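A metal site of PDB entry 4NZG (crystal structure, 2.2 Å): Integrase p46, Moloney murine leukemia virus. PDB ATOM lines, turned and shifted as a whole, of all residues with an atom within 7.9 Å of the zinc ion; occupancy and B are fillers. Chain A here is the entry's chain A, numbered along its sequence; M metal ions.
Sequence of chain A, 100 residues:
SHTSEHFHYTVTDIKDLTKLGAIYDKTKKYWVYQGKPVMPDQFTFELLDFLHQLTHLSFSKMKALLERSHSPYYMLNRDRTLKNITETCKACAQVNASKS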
ATOM      1  N   ASP A  49       2.066 -34.836  23.618  1.00  0.00           N
ATOM      2  CA  ASP A  49       2.502 -33.508  24.037  1.00  0.00           C
ATOM      3  C   ASP A  49       2.444 -32.566  22.843  1.00  0.00           C
ATOM      4  O   ASP A  49       1.953 -31.436  22.953  1.00  0.00           O
ATOM      5  CB  ASP A  49       3.921 -33.558  24.600  1.00  0.00           C
ATOM      6  CG  ASP A  49       4.431 -32.198  25.040  1.00  0.00           C
ATOM      7  OD1 ASP A  49       3.998 -31.710  26.107  1.00  0.00           O
ATOM      8  OD2 ASP A  49       5.287 -31.615  24.335  1.00  0.00           O
ATOM      9  N   HIS A  52      -1.283 -31.780  22.037  1.00  0.00           N
ATOM     10  CA  HIS A  52      -1.881 -30.858  23.002  1.00  0.00           C
ATOM     11  C   HIS A  52      -1.413 -29.421  22.784  1.00  0.00           C
ATOM     12  O   HIS A  52      -2.182 -28.486  22.964  1.00  0.00           O
ATOM     13  CB  HIS A  52      -1.583 -31.293  24.439  1.00  0.00           C
ATOM     14  CG  HIS A  52      -2.175 -30.370  25.471  1.00  0.00           C
ATOM     15  ND1 HIS A  52      -3.459 -30.517  25.955  1.00  0.00           N
ATOM     16  CD2 HIS A  52      -1.655 -29.291  26.106  1.00  0.00           C
ATOM     17  CE1 HIS A  52      -3.712 -29.570  26.841  1.00  0.00           C
ATOM     18  NE2 HIS A  52      -2.628 -28.809  26.951  1.00  0.00           N
ATOM     19  N   GLN A  53      -0.149 -29.246  22.401  1.00  0.00           N
ATOM     20  CA  GLN A  53       0.382 -27.902  22.205  1.00  0.00           C
ATOM     21  C   GLN A  53      -0.341 -27.161  21.083  1.00  0.00           C
ATOM     22  O   GLN A  53      -0.455 -25.937  21.108  1.00  0.00           O
ATOM     23  CB  GLN A  53       1.886 -27.943  21.921  1.00  0.00           C
ATOM     24  CG  GLN A  53       2.732 -28.485  23.073  1.00  0.00           C
ATOM     25  CD  GLN A  53       2.516 -27.726  24.373  1.00  0.00           C
ATOM     26  OE1 GLN A  53       2.488 -26.495  24.387  1.00  0.00           O
ATOM     27  NE2 GLN A  53       2.358 -28.466  25.459  1.00  0.00           N
ATOM     28  N   LEU A  54      -0.835 -27.914  20.097  1.00  0.00           N
ATOM     29  CA  LEU A  54      -1.553 -27.332  18.970  1.00  0.00           C
ATOM     30  C   LEU A  54      -3.044 -27.116  19.224  1.00  0.00           C
ATOM     31  O   LEU A  54      -3.687 -26.383  18.484  1.00  0.00           O
ATOM     32  CB  LEU A  54      -1.369 -28.187  17.697  1.00  0.00           C
ATOM     33  CG  LEU A  54      -0.065 -28.028  16.891  1.00  0.00           C
ATOM     34  CD1 LEU A  54       1.128 -28.590  17.597  1.00  0.00           C
ATOM     35  CD2 LEU A  54      -0.210 -28.683  15.526  1.00  0.00           C
ATOM     36  N   THR A  55      -3.591 -27.748  20.250  1.00  0.00           N
ATOM     37  CA  THR A  55      -5.036 -27.711  20.465  1.00  0.00           C
ATOM     38  C   THR A  55      -5.421 -27.300  21.882  1.00  0.00           C
ATOM     39  O   THR A  55      -6.455 -26.671  22.102  1.00  0.00           O
ATOM     40  CB  THR A  55      -5.679 -29.089  20.188  1.00  0.00           C
ATOM     41  OG1 THR A  55      -5.193 -30.032  21.147  1.00  0.00           O
ATOM     42  CG2 THR A  55      -5.345 -29.568  18.786  1.00  0.00           C
ATOM     43  N   HIS A  56      -4.581 -27.679  22.838  1.00  0.00           N
ATOM     44  CA  HIS A  56      -4.833 -27.458  24.268  1.00  0.00           C
ATOM     45  C   HIS A  56      -6.198 -27.974  24.694  1.00  0.00           C
ATOM     46  O   HIS A  56      -6.872 -27.380  25.523  1.00  0.00           O
ATOM     47  CB  HIS A  56      -4.665 -25.979  24.608  1.00  0.00           C
ATOM     48  CG  HIS A  56      -3.234 -25.537  24.582  1.00  0.00           C
ATOM     49  ND1 HIS A  56      -2.337 -25.902  25.557  1.00  0.00           N
ATOM     50  CD2 HIS A  56      -2.550 -24.789  23.684  1.00  0.00           C
ATOM     51  CE1 HIS A  56      -1.150 -25.386  25.262  1.00  0.00           C
ATOM     52  NE2 HIS A  56      -1.249 -24.710  24.141  1.00  0.00           N
ATOM     53  N   LEU A  57      -6.593 -29.104  24.107  1.00  0.00           N
ATOM     54  CA  LEU A  57      -7.817 -29.772  24.518  1.00  0.00           C
ATOM     55  C   LEU A  57      -7.591 -30.433  25.872  1.00  0.00           C
ATOM     56  O   LEU A  57      -6.495 -30.909  26.155  1.00  0.00           O
ATOM     57  CB  LEU A  57      -8.248 -30.796  23.468  1.00  0.00           C
ATOM     58  CG  LEU A  57      -8.719 -30.210  22.149  1.00  0.00           C
ATOM     59  CD1 LEU A  57      -8.742 -31.275  21.058  1.00  0.00           C
ATOM     60  CD2 LEU A  57     -10.092 -29.578  22.306  1.00  0.00           C
ATOM     61  N   SER A  58      -8.637 -30.487  26.680  1.00  0.00           N
ATOM     62  CA  SER A  58      -8.543 -31.072  28.009  1.00  0.00           C
ATOM     63  C   SER A  58      -8.291 -32.576  27.937  1.00  0.00           C
ATOM     64  O   SER A  58      -8.320 -33.165  26.853  1.00  0.00           O
ATOM     65  CB  SER A  58      -9.807 -30.783  28.814  1.00  0.00           C
ATOM     66  OG  SER A  58     -10.922 -31.465  28.255  1.00  0.00           O
ATOM     67  N   MET A  62      -9.310 -34.995  24.638  1.00  0.00           N
ATOM     68  CA  MET A  62      -8.232 -35.690  23.944  1.00  0.00           C
ATOM     69  C   MET A  62      -8.406 -37.211  24.018  1.00  0.00           C
ATOM     70  O   MET A  62      -8.226 -37.907  23.011  1.00  0.00           O
ATOM     71  CB  MET A  62      -6.874 -35.296  24.520  1.00  0.00           C
ATOM     72  CG  MET A  62      -6.453 -33.867  24.216  1.00  0.00           C
ATOM     73  SD  MET A  62      -4.718 -33.543  24.611  1.00  0.00           S
ATOM     74  CE  MET A  62      -3.900 -34.403  23.267  1.00  0.00           C
ATOM     75  N   ILE A  85       0.368 -34.504  31.013  1.00  0.00           N
ATOM     76  CA  ILE A  85       0.557 -33.449  30.028  1.00  0.00           C
ATOM     77  C   ILE A  85      -0.434 -32.300  30.209  1.00  0.00           C
ATOM     78  O   ILE A  85      -0.049 -31.122  30.222  1.00  0.00           O
ATOM     79  CB  ILE A  85       0.436 -34.005  28.594  1.00  0.00           C
ATOM     80  CG1 ILE A  85       1.643 -34.908  28.279  1.00  0.00           C
ATOM     81  CG2 ILE A  85       0.351 -32.868  27.592  1.00  0.00           C
ATOM     82  CD1 ILE A  85       1.539 -35.610  26.938  1.00  0.00           C
ATOM     83  N   THR A  86      -1.713 -32.632  30.374  1.00  0.00           N
ATOM     84  CA  THR A  86      -2.747 -31.622  30.480  1.00  0.00           C
ATOM     85  C   THR A  86      -2.716 -30.887  31.834  1.00  0.00           C
ATOM     86  O   THR A  86      -3.003 -29.689  31.891  1.00  0.00           O
ATOM     87  CB  THR A  86      -4.157 -32.233  30.263  1.00  0.00           C
ATOM     88  OG1 THR A  86      -4.352 -33.330  31.175  1.00  0.00           O
ATOM     89  CG2 THR A  86      -4.284 -32.749  28.841  1.00  0.00           C
ATOM     90  N   GLU A  87      -2.335 -31.594  32.897  1.00  0.00           N
ATOM     91  CA  GLU A  87      -2.337 -31.006  34.232  1.00  0.00           C
ATOM     92  C   GLU A  87      -1.101 -30.149  34.529  1.00  0.00           C
ATOM     93  O   GLU A  87      -1.081 -29.362  35.482  1.00  0.00           O
ATOM     94  CB  GLU A  87      -2.480 -32.120  35.281  1.00  0.00           C
ATOM     95  CG  GLU A  87      -2.486 -31.673  36.745  1.00  0.00           C
ATOM     96  CD  GLU A  87      -3.489 -30.566  37.012  1.00  0.00           C
ATOM     97  OE1 GLU A  87      -4.614 -30.628  36.476  1.00  0.00           O
ATOM     98  OE2 GLU A  87      -3.138 -29.630  37.754  1.00  0.00           O
ATOM     99  N   THR A  88      -0.076 -30.253  33.697  1.00  0.00           N
ATOM    100  CA  THR A  88       1.118 -29.440  33.882  1.00  0.00           C
ATOM    101  C   THR A  88       1.270 -28.388  32.783  1.00  0.00           C
ATOM    102  O   THR A  88       2.260 -27.670  32.743  1.00  0.00           O
ATOM    103  CB  THR A  88       2.411 -30.294  33.936  1.00  0.00           C
ATOM    104  OG1 THR A  88       2.621 -30.945  32.671  1.00  0.00           O
ATOM    105  CG2 THR A  88       2.319 -31.340  35.044  1.00  0.00           C
ATOM    106  N   CYS A  89       0.281 -28.303  31.891  1.00  0.00           N
ATOM    107  CA  CYS A  89       0.333 -27.296  30.836  1.00  0.00           C
ATOM    108  C   CYS A  89       0.137 -25.912  31.446  1.00  0.00           C
ATOM    109  O   CYS A  89      -0.868 -25.646  32.102  1.00  0.00           O
ATOM    110  CB  CYS A  89      -0.726 -27.537  29.763  1.00  0.00           C
ATOM    111  SG  CYS A  89      -0.670 -26.280  28.457  1.00  0.00           S
ATOM    112  N   LYS A  90       1.120 -25.056  31.219  1.00  0.00           N
ATOM    113  CA  LYS A  90       1.132 -23.708  31.765  1.00  0.00           C
ATOM    114  C   LYS A  90       0.012 -22.841  31.166  1.00  0.00           C
ATOM    115  O   LYS A  90      -0.722 -22.172  31.885  1.00  0.00           O
ATOM    116  CB  LYS A  90       2.499 -23.073  31.518  1.00  0.00           C
ATOM    117  CG  LYS A  90       2.668 -21.652  32.026  1.00  0.00           C
ATOM    118  CD  LYS A  90       4.059 -21.150  31.667  1.00  0.00           C
ATOM    119  CE  LYS A  90       4.224 -19.693  32.015  1.00  0.00           C
ATOM    120  NZ  LYS A  90       4.051 -19.476  33.476  1.00  0.00           N
ATOM    121  N   ALA A  91      -0.095 -22.881  29.846  1.00  0.00           N
ATOM    122  CA  ALA A  91      -1.101 -22.108  29.119  1.00  0.00           C
ATOM    123  C   ALA A  91      -2.521 -22.452  29.577  1.00  0.00           C
ATOM    124  O   ALA A  91      -3.332 -21.565  29.807  1.00  0.00           O
ATOM    125  CB  ALA A  91      -0.957 -22.330  27.622  1.00  0.00           C
ATOM    126  N   CYS A  92      -2.827 -23.747  29.696  1.00  0.00           N
ATOM    127  CA  CYS A  92      -4.141 -24.167  30.159  1.00  0.00           C
ATOM    128  C   CYS A  92      -4.371 -23.733  31.607  1.00  0.00           C
ATOM    129  O   CYS A  92      -5.488 -23.350  31.971  1.00  0.00           O
ATOM    130  CB  CYS A  92      -4.309 -25.687  30.039  1.00  0.00           C
ATOM    131  SG  CYS A  92      -4.553 -26.293  28.345  1.00  0.00           S
ATOM    132  N   ALA A  93      -3.325 -23.776  32.421  1.00  0.00           N
ATOM    133  CA  ALA A  93      -3.404 -23.311  33.797  1.00  0.00           C
ATOM    134  C   ALA A  93      -3.738 -21.821  33.831  1.00  0.00           C
ATOM    135  O   ALA A  93      -4.502 -21.361  34.677  1.00  0.00           O
ATOM    136  CB  ALA A  93      -2.106 -23.577  34.542  1.00  0.00           C
ATOM    137  N   VAL A  95      -5.318 -20.213  31.429  1.00  0.00           N
ATOM    138  CA  VAL A  95      -6.696 -20.102  30.954  1.00  0.00           C
ATOM    139  C   VAL A  95      -7.721 -20.269  32.075  1.00  0.00           C
ATOM    140  O   VAL A  95      -8.585 -19.419  32.249  1.00  0.00           O
ATOM    141  CB  VAL A  95      -6.994 -21.138  29.851  1.00  0.00           C
ATOM    142  CG1 VAL A  95      -8.493 -21.270  29.617  1.00  0.00           C
ATOM    143  CG2 VAL A  95      -6.290 -20.760  28.558  1.00  0.00           C
HETATM  144 ZN    ZN M   1      -2.606 -26.800  27.365  1.00  0.00          ZN
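Four residues have an atom within 4 Å of the zinc ion: His 52, His 56, Cys 89 and Cys 92. The nearest printed residue that does not touch the zinc ion is Ala 91 (4.8 Å).
A ring nitrogen (NE2) of His 56 sits at hydrogen-bond distance from the backbone carbonyl oxygen (O) of Gln 53. A ring nitrogen (ND1) of His 52 is in hydrogen-bond range of the backbone carbonyl oxygen of Leu 57, at 3.1 Å. ND1 of His 52 is in hydrogen-bond range of SD of Met 62 (3.5 Å). The backbone NH (N) of Ala 91 lies close to the side-chain sulfur (SG) of Cys 89 (3.7 Å).
The zinc ion is bound by ND1 of His 56. The zinc ion is bound by NE2 of His 52, at 2.1 Å. The zinc ion is bound by SG of Cys 92, at 2.2 Å. The zinc ion is bound by SG of Cys 89, at 2.3 Å. The zinc ion has four donor atoms within binding distance.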
